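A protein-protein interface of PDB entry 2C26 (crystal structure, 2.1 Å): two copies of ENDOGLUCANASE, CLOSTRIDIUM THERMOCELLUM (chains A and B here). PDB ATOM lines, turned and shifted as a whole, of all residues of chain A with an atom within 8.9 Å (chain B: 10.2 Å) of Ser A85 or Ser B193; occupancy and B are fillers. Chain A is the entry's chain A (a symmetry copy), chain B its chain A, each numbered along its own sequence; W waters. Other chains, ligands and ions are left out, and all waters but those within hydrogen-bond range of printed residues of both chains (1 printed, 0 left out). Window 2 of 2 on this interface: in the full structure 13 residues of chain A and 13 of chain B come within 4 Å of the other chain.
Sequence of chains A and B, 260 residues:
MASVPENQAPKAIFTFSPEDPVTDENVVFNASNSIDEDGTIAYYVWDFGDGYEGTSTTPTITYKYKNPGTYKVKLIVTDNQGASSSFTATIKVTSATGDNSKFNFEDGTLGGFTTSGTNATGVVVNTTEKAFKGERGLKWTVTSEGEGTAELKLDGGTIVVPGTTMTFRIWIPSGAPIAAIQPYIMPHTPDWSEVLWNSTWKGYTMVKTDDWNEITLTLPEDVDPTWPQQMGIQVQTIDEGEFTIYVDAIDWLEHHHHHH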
ATOM      1  N   GLN A   8     -20.049  13.506  17.453  1.00  0.00           N
ATOM      2  CA  GLN A   8     -19.180  13.997  18.503  1.00  0.00           C
ATOM      3  C   GLN A   8     -19.863  15.158  19.206  1.00  0.00           C
ATOM      4  O   GLN A   8     -20.394  16.056  18.557  1.00  0.00           O
ATOM      5  CB  GLN A   8     -17.832  14.418  17.907  1.00  0.00           C
ATOM      6  CG  GLN A   8     -16.735  14.722  18.930  1.00  0.00           C
ATOM      7  CD  GLN A   8     -15.421  15.093  18.260  1.00  0.00           C
ATOM      8  OE1 GLN A   8     -14.763  16.064  18.639  1.00  0.00           O
ATOM      9  NE2 GLN A   8     -15.048  14.334  17.248  1.00  0.00           N
ATOM     10  N   ALA A   9     -19.857  15.133  20.534  1.00  0.00           N
ATOM     11  CA  ALA A   9     -20.443  16.216  21.325  1.00  0.00           C
ATOM     12  C   ALA A   9     -19.592  17.485  21.192  1.00  0.00           C
ATOM     13  O   ALA A   9     -18.381  17.398  20.955  1.00  0.00           O
ATOM     14  CB  ALA A   9     -20.602  15.791  22.795  1.00  0.00           C
ATOM     15  N   PRO A  10     -20.230  18.671  21.287  1.00  0.00           N
ATOM     16  CA  PRO A  10     -19.502  19.941  21.174  1.00  0.00           C
ATOM     17  C   PRO A  10     -18.581  20.286  22.357  1.00  0.00           C
ATOM     18  O   PRO A  10     -18.762  19.779  23.465  1.00  0.00           O
ATOM     19  CB  PRO A  10     -20.626  20.974  21.069  1.00  0.00           C
ATOM     20  CG  PRO A  10     -21.800  20.314  21.797  1.00  0.00           C
ATOM     21  CD  PRO A  10     -21.689  18.876  21.437  1.00  0.00           C
ATOM     22  N   LYS A  11     -17.607  21.154  22.092  1.00  0.00           N
ATOM     23  CA  LYS A  11     -16.782  21.786  23.113  1.00  0.00           C
ATOM     24  C   LYS A  11     -17.563  22.981  23.677  1.00  0.00           C
ATOM     25  O   LYS A  11     -17.960  23.853  22.923  1.00  0.00           O
ATOM     26  CB  LYS A  11     -15.450  22.260  22.489  1.00  0.00           C
ATOM     27  CG  LYS A  11     -14.548  23.050  23.447  1.00  0.00           C
ATOM     28  CD  LYS A  11     -13.476  23.887  22.736  1.00  0.00           C
ATOM     29  CE  LYS A  11     -12.413  23.030  22.085  1.00  0.00           C
ATOM     30  NZ  LYS A  11     -11.392  23.875  21.402  1.00  0.00           N
ATOM     31  N   ALA A  12     -17.790  22.997  24.989  1.00  0.00           N
ATOM     32  CA  ALA A  12     -18.459  24.098  25.677  1.00  0.00           C
ATOM     33  C   ALA A  12     -17.502  24.805  26.631  1.00  0.00           C
ATOM     34  O   ALA A  12     -16.867  24.173  27.477  1.00  0.00           O
ATOM     35  CB  ALA A  12     -19.686  23.596  26.440  1.00  0.00           C
ATOM     36  N   ILE A  13     -17.417  26.124  26.490  1.00  0.00           N
ATOM     37  CA  ILE A  13     -16.567  26.965  27.326  1.00  0.00           C
ATOM     38  C   ILE A  13     -17.020  28.407  27.144  1.00  0.00           C
ATOM     39  O   ILE A  13     -17.558  28.756  26.096  1.00  0.00           O
ATOM     40  CB  ILE A  13     -15.042  26.805  26.981  1.00  0.00           C
ATOM     41  CG1 ILE A  13     -14.163  27.494  28.041  1.00  0.00           C
ATOM     42  CG2 ILE A  13     -14.720  27.285  25.552  1.00  0.00           C
ATOM     43  CD1 ILE A  13     -12.831  26.859  28.224  1.00  0.00           C
ATOM     44  N   SER A  34     -16.375  28.030  22.197  1.00  0.00           N
ATOM     45  CA  SER A  34     -17.151  26.805  22.050  1.00  0.00           C
ATOM     46  C   SER A  34     -17.189  26.448  20.575  1.00  0.00           C
ATOM     47  O   SER A  34     -17.178  27.332  19.725  1.00  0.00           O
ATOM     48  CB  SER A  34     -18.589  26.967  22.567  1.00  0.00           C
ATOM     49  OG  SER A  34     -18.618  27.375  23.910  1.00  0.00           O
ATOM     50  N   ILE A  35     -17.252  25.151  20.283  1.00  0.00           N
ATOM     51  CA  ILE A  35     -17.237  24.667  18.904  1.00  0.00           C
ATOM     52  C   ILE A  35     -17.756  23.234  18.842  1.00  0.00           C
ATOM     53  O   ILE A  35     -17.504  22.425  19.739  1.00  0.00           O
ATOM     54  CB  ILE A  35     -15.810  24.779  18.249  1.00  0.00           C
ATOM     55  CG1 ILE A  35     -15.777  24.192  16.829  1.00  0.00           C
ATOM     56  CG2 ILE A  35     -14.701  24.142  19.141  1.00  0.00           C
ATOM     57  CD1 ILE A  35     -14.629  24.755  15.932  1.00  0.00           C
ATOM     58  N   ASP A  36     -18.486  22.934  17.778  1.00  0.00           N
ATOM     59  CA  ASP A  36     -18.790  21.557  17.441  1.00  0.00           C
ATOM     60  C   ASP A  36     -17.851  21.148  16.312  1.00  0.00           C
ATOM     61  O   ASP A  36     -17.896  21.731  15.230  1.00  0.00           O
ATOM     62  CB  ASP A  36     -20.252  21.395  17.022  1.00  0.00           C
ATOM     63  CG  ASP A  36     -20.641  19.942  16.879  1.00  0.00           C
ATOM     64  OD1 ASP A  36     -20.168  19.131  17.696  1.00  0.00           O
ATOM     65  OD2 ASP A  36     -21.410  19.586  15.961  1.00  0.00           O
ATOM     66  N   ILE A  41     -23.061  24.507  16.156  1.00  0.00           N
ATOM     67  CA  ILE A  41     -23.785  24.750  17.408  1.00  0.00           C
ATOM     68  C   ILE A  41     -25.182  25.270  17.109  1.00  0.00           C
ATOM     69  O   ILE A  41     -25.342  26.242  16.363  1.00  0.00           O
ATOM     70  CB  ILE A  41     -23.030  25.708  18.359  1.00  0.00           C
ATOM     71  CG1 ILE A  41     -21.680  25.091  18.760  1.00  0.00           C
ATOM     72  CG2 ILE A  41     -23.902  26.061  19.609  1.00  0.00           C
ATOM     73  CD1 ILE A  41     -20.776  26.014  19.520  1.00  0.00           C
ATOM     74  N   TYR A  43     -27.683  25.623  19.876  1.00  0.00           N
ATOM     75  CA  TYR A  43     -28.167  26.358  21.052  1.00  0.00           C
ATOM     76  C   TYR A  43     -27.034  26.730  22.000  1.00  0.00           C
ATOM     77  O   TYR A  43     -26.185  25.894  22.307  1.00  0.00           O
ATOM     78  CB  TYR A  43     -29.210  25.535  21.841  1.00  0.00           C
ATOM     79  CG  TYR A  43     -30.530  25.317  21.127  1.00  0.00           C
ATOM     80  CD1 TYR A  43     -30.705  24.222  20.283  1.00  0.00           C
ATOM     81  CD2 TYR A  43     -31.610  26.196  21.310  1.00  0.00           C
ATOM     82  CE1 TYR A  43     -31.905  24.013  19.618  1.00  0.00           C
ATOM     83  CE2 TYR A  43     -32.827  25.990  20.650  1.00  0.00           C
ATOM     84  CZ  TYR A  43     -32.957  24.893  19.803  1.00  0.00           C
ATOM     85  OH  TYR A  43     -34.131  24.653  19.135  1.00  0.00           O
ATOM     86  N   TYR A  44     -27.021  27.985  22.446  1.00  0.00           N
ATOM     87  CA  TYR A  44     -26.282  28.385  23.643  1.00  0.00           C
ATOM     88  C   TYR A  44     -27.323  28.639  24.723  1.00  0.00           C
ATOM     89  O   TYR A  44     -28.089  29.608  24.626  1.00  0.00           O
ATOM     90  CB  TYR A  44     -25.491  29.677  23.405  1.00  0.00           C
ATOM     91  CG  TYR A  44     -24.458  29.591  22.320  1.00  0.00           C
ATOM     92  CD1 TYR A  44     -24.786  29.895  20.988  1.00  0.00           C
ATOM     93  CD2 TYR A  44     -23.147  29.212  22.614  1.00  0.00           C
ATOM     94  CE1 TYR A  44     -23.838  29.812  19.993  1.00  0.00           C
ATOM     95  CE2 TYR A  44     -22.192  29.123  21.626  1.00  0.00           C
ATOM     96  CZ  TYR A  44     -22.536  29.424  20.319  1.00  0.00           C
ATOM     97  OH  TYR A  44     -21.575  29.342  19.337  1.00  0.00           O
ATOM     98  N   VAL A  45     -27.391  27.766  25.733  1.00  0.00           N
ATOM     99  CA  VAL A  45     -28.352  27.958  26.825  1.00  0.00           C
ATOM    100  C   VAL A  45     -27.599  28.392  28.079  1.00  0.00           C
ATOM    101  O   VAL A  45     -26.630  27.751  28.489  1.00  0.00           O
ATOM    102  CB  VAL A  45     -29.222  26.685  27.097  1.00  0.00           C
ATOM    103  CG1 VAL A  45     -30.248  26.946  28.220  1.00  0.00           C
ATOM    104  CG2 VAL A  45     -29.936  26.231  25.836  1.00  0.00           C
ATOM    105  N   LYS A  74     -23.934  28.520  34.317  1.00  0.00           N
ATOM    106  CA  LYS A  74     -23.814  27.321  33.516  1.00  0.00           C
ATOM    107  C   LYS A  74     -24.183  27.591  32.061  1.00  0.00           C
ATOM    108  O   LYS A  74     -25.263  28.105  31.767  1.00  0.00           O
ATOM    109  CB  LYS A  74     -24.710  26.213  34.084  1.00  0.00           C
ATOM    110  CG  LYS A  74     -24.625  24.914  33.335  1.00  0.00           C
ATOM    111  CD  LYS A  74     -25.666  23.965  33.844  1.00  0.00           C
ATOM    112  CE  LYS A  74     -25.211  22.549  33.679  1.00  0.00           C
ATOM    113  NZ  LYS A  74     -26.333  21.593  33.958  1.00  0.00           N
ATOM    114  N   LEU A  75     -23.271  27.241  31.163  1.00  0.00           N
ATOM    115  CA  LEU A  75     -23.556  27.222  29.743  1.00  0.00           C
ATOM    116  C   LEU A  75     -23.762  25.782  29.304  1.00  0.00           C
ATOM    117  O   LEU A  75     -22.958  24.910  29.634  1.00  0.00           O
ATOM    118  CB  LEU A  75     -22.384  27.844  28.960  1.00  0.00           C
ATOM    119  CG  LEU A  75     -22.294  27.615  27.443  1.00  0.00           C
ATOM    120  CD1 LEU A  75     -23.383  28.387  26.674  1.00  0.00           C
ATOM    121  CD2 LEU A  75     -20.892  27.951  26.914  1.00  0.00           C
ATOM    122  N   ILE A  76     -24.844  25.524  28.577  1.00  0.00           N
ATOM    123  CA  ILE A  76     -24.966  24.276  27.836  1.00  0.00           C
ATOM    124  C   ILE A  76     -24.926  24.602  26.349  1.00  0.00           C
ATOM    125  O   ILE A  76     -25.643  25.479  25.876  1.00  0.00           O
ATOM    126  CB  ILE A  76     -26.231  23.445  28.190  1.00  0.00           C
ATOM    127  CG1 ILE A  76     -26.223  23.073  29.675  1.00  0.00           C
ATOM    128  CG2 ILE A  76     -26.270  22.157  27.339  1.00  0.00           C
ATOM    129  CD1 ILE A  76     -27.541  22.419  30.191  1.00  0.00           C
ATOM    130  N   VAL A  77     -24.041  23.917  25.640  1.00  0.00           N
ATOM    131  CA  VAL A  77     -23.906  24.045  24.195  1.00  0.00           C
ATOM    132  C   VAL A  77     -24.498  22.777  23.600  1.00  0.00           C
ATOM    133  O   VAL A  77     -24.138  21.682  24.022  1.00  0.00           O
ATOM    134  CB  VAL A  77     -22.400  24.198  23.778  1.00  0.00           C
ATOM    135  CG1 VAL A  77     -22.235  24.069  22.273  1.00  0.00           C
ATOM    136  CG2 VAL A  77     -21.863  25.538  24.237  1.00  0.00           C
ATOM    137  N   THR A  78     -25.416  22.931  22.643  1.00  0.00           N
ATOM    138  CA  THR A  78     -26.060  21.801  21.983  1.00  0.00           C
ATOM    139  C   THR A  78     -25.800  21.895  20.485  1.00  0.00           C
ATOM    140  O   THR A  78     -25.992  22.951  19.896  1.00  0.00           O
ATOM    141  CB  THR A  78     -27.593  21.775  22.270  1.00  0.00           C
ATOM    142  OG1 THR A  78     -27.817  21.744  23.687  1.00  0.00           O
ATOM    143  CG2 THR A  78     -28.265  20.556  21.637  1.00  0.00           C
ATOM    144  N   ASP A  79     -25.356  20.800  19.876  1.00  0.00           N
ATOM    145  CA  ASP A  79     -25.031  20.815  18.453  1.00  0.00           C
ATOM    146  C   ASP A  79     -26.261  20.551  17.569  1.00  0.00           C
ATOM    147  O   ASP A  79     -27.381  20.372  18.080  1.00  0.00           O
ATOM    148  CB  ASP A  79     -23.849  19.873  18.128  1.00  0.00           C
ATOM    149  CG  ASP A  79     -24.190  18.384  18.263  1.00  0.00           C
ATOM    150  OD1 ASP A  79     -25.365  18.000  18.298  1.00  0.00           O
ATOM    151  OD2 ASP A  79     -23.252  17.569  18.341  1.00  0.00           O
ATOM    152  N   GLY A  82     -28.309  17.411  18.505  1.00  0.00           N
ATOM    153  CA  GLY A  82     -28.895  17.282  19.832  1.00  0.00           C
ATOM    154  C   GLY A  82     -27.940  16.838  20.923  1.00  0.00           C
ATOM    155  O   GLY A  82     -28.368  16.642  22.053  1.00  0.00           O
ATOM    156  N   ALA A  83     -26.653  16.682  20.592  1.00  0.00           N
ATOM    157  CA  ALA A  83     -25.626  16.352  21.591  1.00  0.00           C
ATOM    158  C   ALA A  83     -25.175  17.614  22.330  1.00  0.00           C
ATOM    159  O   ALA A  83     -25.024  18.681  21.719  1.00  0.00           O
ATOM    160  CB  ALA A  83     -24.437  15.643  20.954  1.00  0.00           C
ATOM    161  N   SER A  84     -24.973  17.499  23.639  1.00  0.00           N
ATOM    162  CA  SER A  84     -24.621  18.665  24.437  1.00  0.00           C
ATOM    163  C   SER A  84     -23.436  18.440  25.381  1.00  0.00           C
ATOM    164  O   SER A  84     -23.137  17.302  25.770  1.00  0.00           O
ATOM    165  CB  SER A  84     -25.835  19.130  25.239  1.00  0.00           C
ATOM    166  OG  SER A  84     -26.236  18.086  26.106  1.00  0.00           O
ATOM    167  N   SER A  85     -22.777  19.545  25.726  1.00  0.00           N
ATOM    168  CA  SER A  85     -21.743  19.602  26.752  1.00  0.00           C
ATOM    169  C   SER A  85     -22.001  20.850  27.575  1.00  0.00           C
ATOM    170  O   SER A  85     -22.594  21.823  27.082  1.00  0.00           O
ATOM    171  CB  SER A  85     -20.344  19.725  26.125  1.00  0.00           C
ATOM    172  OG  SER A  85     -20.034  18.615  25.289  1.00  0.00           O
ATOM    173  N   SER A  86     -21.539  20.840  28.819  1.00  0.00           N
ATOM    174  CA  SER A  86     -21.721  22.003  29.674  1.00  0.00           C
ATOM    175  C   SER A  86     -20.424  22.483  30.327  1.00  0.00           C
ATOM    176  O   SER A  86     -19.468  21.724  30.492  1.00  0.00           O
ATOM    177  CB  SER A  86     -22.812  21.750  30.729  1.00  0.00           C
ATOM    178  OG  SER A  86     -22.342  20.895  31.758  1.00  0.00           O
ATOM    179  N   PHE A  87     -20.425  23.759  30.699  1.00  0.00           N
ATOM    180  CA  PHE A  87     -19.295  24.401  31.344  1.00  0.00           C
ATOM    181  C   PHE A  87     -19.876  25.357  32.361  1.00  0.00           C
ATOM    182  O   PHE A  87     -20.706  26.199  32.016  1.00  0.00           O
ATOM    183  CB  PHE A  87     -18.451  25.161  30.312  1.00  0.00           C
ATOM    184  CG  PHE A  87     -17.185  25.744  30.878  1.00  0.00           C
ATOM    185  CD1 PHE A  87     -17.164  27.038  31.391  1.00  0.00           C
ATOM    186  CD2 PHE A  87     -16.011  24.993  30.911  1.00  0.00           C
ATOM    187  CE1 PHE A  87     -15.980  27.575  31.912  1.00  0.00           C
ATOM    188  CE2 PHE A  87     -14.845  25.511  31.429  1.00  0.00           C
ATOM    189  CZ  PHE A  87     -14.819  26.807  31.927  1.00  0.00           C
ATOM    190  N   THR A  88     -19.460  25.222  33.612  1.00  0.00           N
ATOM    191  CA  THR A  88     -19.989  26.051  34.683  1.00  0.00           C
ATOM    192  C   THR A  88     -18.844  26.811  35.346  1.00  0.00           C
ATOM    193  O   THR A  88     -17.847  26.201  35.750  1.00  0.00           O
ATOM    194  CB  THR A  88     -20.753  25.196  35.744  1.00  0.00           C
ATOM    195  OG1 THR A  88     -21.800  24.461  35.110  1.00  0.00           O
ATOM    196  CG2 THR A  88     -21.337  26.053  36.866  1.00  0.00           C
ATOM    197  N   PRO B 187     -13.010  20.391  38.312  1.00  0.00           N
ATOM    198  CA  PRO B 187     -13.758  19.129  38.362  1.00  0.00           C
ATOM    199  C   PRO B 187     -14.524  18.918  37.057  1.00  0.00           C
ATOM    200  O   PRO B 187     -14.942  19.879  36.417  1.00  0.00           O
ATOM    201  CB  PRO B 187     -14.766  19.345  39.498  1.00  0.00           C
ATOM    202  CG  PRO B 187     -14.250  20.493  40.274  1.00  0.00           C
ATOM    203  CD  PRO B 187     -13.472  21.342  39.343  1.00  0.00           C
ATOM    204  N   HIS B 188     -14.697  17.667  36.671  1.00  0.00           N
ATOM    205  CA  HIS B 188     -15.355  17.338  35.422  1.00  0.00           C
ATOM    206  C   HIS B 188     -15.875  15.911  35.574  1.00  0.00           C
ATOM    207  O   HIS B 188     -15.335  15.136  36.375  1.00  0.00           O
ATOM    208  CB  HIS B 188     -14.373  17.472  34.234  1.00  0.00           C
ATOM    209  CG  HIS B 188     -13.133  16.638  34.374  1.00  0.00           C
ATOM    210  ND1 HIS B 188     -13.064  15.329  33.945  1.00  0.00           N
ATOM    211  CD2 HIS B 188     -11.926  16.916  34.923  1.00  0.00           C
ATOM    212  CE1 HIS B 188     -11.867  14.839  34.216  1.00  0.00           C
ATOM    213  NE2 HIS B 188     -11.159  15.780  34.815  1.00  0.00           N
ATOM    214  N   THR B 189     -16.922  15.558  34.841  1.00  0.00           N
ATOM    215  CA  THR B 189     -17.337  14.164  34.799  1.00  0.00           C
ATOM    216  C   THR B 189     -16.204  13.368  34.114  1.00  0.00           C
ATOM    217  O   THR B 189     -15.413  13.942  33.357  1.00  0.00           O
ATOM    218  CB  THR B 189     -18.670  13.970  34.039  1.00  0.00           C
ATOM    219  OG1 THR B 189     -18.550  14.533  32.733  1.00  0.00           O
ATOM    220  CG2 THR B 189     -19.855  14.622  34.783  1.00  0.00           C
ATOM    221  N   PRO B 190     -16.096  12.058  34.398  1.00  0.00           N
ATOM    222  CA  PRO B 190     -15.098  11.234  33.689  1.00  0.00           C
ATOM    223  C   PRO B 190     -15.134  11.378  32.153  1.00  0.00           C
ATOM    224  O   PRO B 190     -14.088  11.378  31.507  1.00  0.00           O
ATOM    225  CB  PRO B 190     -15.466   9.811  34.108  1.00  0.00           C
ATOM    226  CG  PRO B 190     -16.115   9.975  35.469  1.00  0.00           C
ATOM    227  CD  PRO B 190     -16.849  11.285  35.411  1.00  0.00           C
ATOM    228  N   ASP B 191     -16.320  11.531  31.570  1.00  0.00           N
ATOM    229  CA  ASP B 191     -16.412  11.684  30.122  1.00  0.00           C
ATOM    230  C   ASP B 191     -16.179  13.113  29.597  1.00  0.00           C
ATOM    231  O   ASP B 191     -16.225  13.334  28.390  1.00  0.00           O
ATOM    232  CB  ASP B 191     -17.712  11.086  29.583  1.00  0.00           C
ATOM    233  CG  ASP B 191     -18.934  11.906  29.933  1.00  0.00           C
ATOM    234  OD1 ASP B 191     -18.851  12.952  30.627  1.00  0.00           O
ATOM    235  OD2 ASP B 191     -20.002  11.496  29.475  1.00  0.00           O
ATOM    236  N   TRP B 192     -15.917  14.055  30.512  1.00  0.00           N
ATOM    237  CA  TRP B 192     -15.681  15.480  30.209  1.00  0.00           C
ATOM    238  C   TRP B 192     -16.880  16.229  29.598  1.00  0.00           C
ATOM    239  O   TRP B 192     -16.723  17.357  29.104  1.00  0.00           O
ATOM    240  CB  TRP B 192     -14.447  15.668  29.307  1.00  0.00           C
ATOM    241  CG  TRP B 192     -13.122  15.526  30.005  1.00  0.00           C
ATOM    242  CD1 TRP B 192     -12.422  14.371  30.218  1.00  0.00           C
ATOM    243  CD2 TRP B 192     -12.335  16.583  30.563  1.00  0.00           C
ATOM    244  NE1 TRP B 192     -11.254  14.647  30.890  1.00  0.00           N
ATOM    245  CE2 TRP B 192     -11.177  15.997  31.110  1.00  0.00           C
ATOM    246  CE3 TRP B 192     -12.513  17.969  30.680  1.00  0.00           C
ATOM    247  CZ2 TRP B 192     -10.173  16.753  31.740  1.00  0.00           C
ATOM    248  CZ3 TRP B 192     -11.517  18.718  31.313  1.00  0.00           C
ATOM    249  CH2 TRP B 192     -10.362  18.105  31.829  1.00  0.00           C
ATOM    250  N   SER B 193     -18.061  15.613  29.634  1.00  0.00           N
ATOM    251  CA  SER B 193     -19.289  16.246  29.120  1.00  0.00           C
ATOM    252  C   SER B 193     -19.768  17.386  30.014  1.00  0.00           C
ATOM    253  O   SER B 193     -20.545  18.233  29.576  1.00  0.00           O
ATOM    254  CB  SER B 193     -20.407  15.209  28.947  1.00  0.00           C
ATOM    255  OG  SER B 193     -20.830  14.706  30.206  1.00  0.00           O
ATOM    256  N   GLU B 194     -19.323  17.392  31.268  1.00  0.00           N
ATOM    257  CA  GLU B 194     -19.669  18.454  32.208  1.00  0.00           C
ATOM    258  C   GLU B 194     -18.421  18.867  32.939  1.00  0.00           C
ATOM    259  O   GLU B 194     -17.750  18.021  33.550  1.00  0.00           O
ATOM    260  CB  GLU B 194     -20.713  17.999  33.230  1.00  0.00           C
ATOM    261  CG  GLU B 194     -21.958  17.411  32.635  1.00  0.00           C
ATOM    262  CD  GLU B 194     -22.947  16.930  33.683  1.00  0.00           C
ATOM    263  OE1 GLU B 194     -23.023  17.521  34.769  1.00  0.00           O
ATOM    264  OE2 GLU B 194     -23.669  15.960  33.412  1.00  0.00           O
ATOM    265  N   VAL B 195     -18.113  20.161  32.865  1.00  0.00           N
ATOM    266  CA  VAL B 195     -16.921  20.751  33.453  1.00  0.00           C
ATOM    267  C   VAL B 195     -17.311  21.882  34.416  1.00  0.00           C
ATOM    268  O   VAL B 195     -18.200  22.679  34.108  1.00  0.00           O
ATOM    269  CB  VAL B 195     -15.972  21.291  32.336  1.00  0.00           C
ATOM    270  CG1 VAL B 195     -14.821  22.064  32.921  1.00  0.00           C
ATOM    271  CG2 VAL B 195     -15.442  20.134  31.453  1.00  0.00           C
ATOM    272  N   LEU B 196     -16.665  21.926  35.586  1.00  0.00           N
ATOM    273  CA  LEU B 196     -16.826  23.017  36.551  1.00  0.00           C
ATOM    274  C   LEU B 196     -15.523  23.788  36.637  1.00  0.00           C
ATOM    275  O   LEU B 196     -14.440  23.203  36.654  1.00  0.00           O
ATOM    276  CB  LEU B 196     -17.203  22.504  37.944  1.00  0.00           C
ATOM    277  CG  LEU B 196     -18.325  21.463  38.074  1.00  0.00           C
ATOM    278  CD1 LEU B 196     -18.453  21.026  39.545  1.00  0.00           C
ATOM    279  CD2 LEU B 196     -19.664  21.980  37.535  1.00  0.00           C
ATOM    280  N   TRP B 227     -16.061  13.339  41.271  1.00  0.00           N
ATOM    281  CA  TRP B 227     -15.555  13.832  39.981  1.00  0.00           C
ATOM    282  C   TRP B 227     -14.036  14.037  39.996  1.00  0.00           C
ATOM    283  O   TRP B 227     -13.495  14.617  40.953  1.00  0.00           O
ATOM    284  CB  TRP B 227     -16.232  15.153  39.598  1.00  0.00           C
ATOM    285  CG  TRP B 227     -17.669  15.044  39.176  1.00  0.00           C
ATOM    286  CD1 TRP B 227     -18.523  13.991  39.380  1.00  0.00           C
ATOM    287  CD2 TRP B 227     -18.428  16.049  38.501  1.00  0.00           C
ATOM    288  NE1 TRP B 227     -19.765  14.280  38.870  1.00  0.00           N
ATOM    289  CE2 TRP B 227     -19.734  15.538  38.321  1.00  0.00           C
ATOM    290  CE3 TRP B 227     -18.132  17.331  38.028  1.00  0.00           C
ATOM    291  CZ2 TRP B 227     -20.743  16.264  37.679  1.00  0.00           C
ATOM    292  CZ3 TRP B 227     -19.145  18.055  37.381  1.00  0.00           C
ATOM    293  CH2 TRP B 227     -20.427  17.518  37.221  1.00  0.00           C
ATOM    294  N   PRO B 228     -13.346  13.543  38.948  1.00  0.00           N
ATOM    295  CA  PRO B 228     -11.921  13.792  38.761  1.00  0.00           C
ATOM    296  C   PRO B 228     -11.674  15.293  38.591  1.00  0.00           C
ATOM    297  O   PRO B 228     -12.571  16.019  38.182  1.00  0.00           O
ATOM    298  CB  PRO B 228     -11.585  13.021  37.478  1.00  0.00           C
ATOM    299  CG  PRO B 228     -12.900  12.782  36.815  1.00  0.00           C
ATOM    300  CD  PRO B 228     -13.892  12.661  37.900  1.00  0.00           C
HETATM  301  O   HOH W   1     -21.043  22.139  33.767  1.00  0.00           O
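No position is printed for both chains.
No residue of chain B comes within 4 Å of Ala A9.
Ala A12 touches none of the printed residues of chain B.
Lys A74 touches none of the printed residues of chain B.
No residue of chain B comes within 4 Å of Ile A76.
Asp A79 touches none of the printed residues of chain B.
No residue of chain B comes within 4 Å of Ser A84.
Ser A85 touches just one residue of chain B: Ser B193.
Of chain B, only Ser B193 (2.9 Å), Glu B194 (3.6 Å) and Val B195 (3.1 Å) come within 4 Å of Ser A86.
Printed residues of chain B within 4 Å of Phe A87: Val B195.
Of the printed residues of chain B, Thr A88 touches Val B195 and Leu B196.
Asp B191 touches none of the printed residues of chain A.
Ser B193 touches two residues of chain A.
Of the printed residues of chain A, Glu B194 touches Ser A86 (3.6 Å).
Of the printed residues of chain A, Val B195 touches Ser A86 (3.1 Å), Phe A87 (3.4 Å) and Thr A88 (2.9 Å).
Of the printed residues of chain A, Leu B196 touches Thr A88 (3.4 Å).
The nearest residue of chain B that does not touch Ser A85 is Trp B192 (5.2 Å).
The nearest residue of chain A that does not touch Ser B193 is Ser A84 (4.7 Å).
The nearest printed residue of chain A that does not touch Glu B194 is Lys A74 (5.3 Å).
Among the printed residues, merely in contact across the chains: Ser A85 with Ser B193, Ser A86 with Glu B194, Phe A87 with Val B195 and Thr A88 with Leu B196.
Water W1 lies within hydrogen-bond range of the side-chain hydroxyl (OG) of Ser A86, the side-chain hydroxyl (OG1) of Thr A88 and the backbone carbonyl oxygen (O) of Val B195.
The backbone NH of Ser A86 lies within hydrogen-bond range of the backbone carbonyl oxygen of Ser B193 (2.9 Å).
N of Val B195 sits at hydrogen-bond distance from O of Ser A86, at 3.1 Å.
O of Val B195 is in hydrogen-bond range of N of Thr A88 (2.9 Å).
O of Pro B187 is in hydrogen-bond range of N of Leu B196.
The backbone NH (N) of Ser B193 lies within hydrogen-bond range of the side-chain hydroxyl (OG1) of Thr B189, 3.3 Å away.
O of Glu B194 sits at hydrogen-bond distance from N of Thr B189 (2.9 Å).
The side-chain carboxylate (OD1) of Asp B191 is in hydrogen-bond range of the side-chain hydroxyl (OG) of Ser B193.
The side-chain hydroxyl (OG) of Ser A85 lies within hydrogen-bond range of the backbone carbonyl oxygen (O) of Pro A10 (2.5 Å).
The backbone NH of Val A77 sits at hydrogen-bond distance from the backbone carbonyl oxygen of Ser A85, 2.9 Å away.
Of the 26 printed residues of chain A, 4 touch a printed residue of chain B.
Hydrophobic or aromatic side chains of chain B within 4 Å of the printed part of chain A: Val B195 and Leu B196.
Among the printed residues, 7 pairs touch across the chains.
Among the printed residues, no Asp or Glu carboxylate lies within 4 Å of a Lys or Arg side-chain nitrogen of the other chain.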
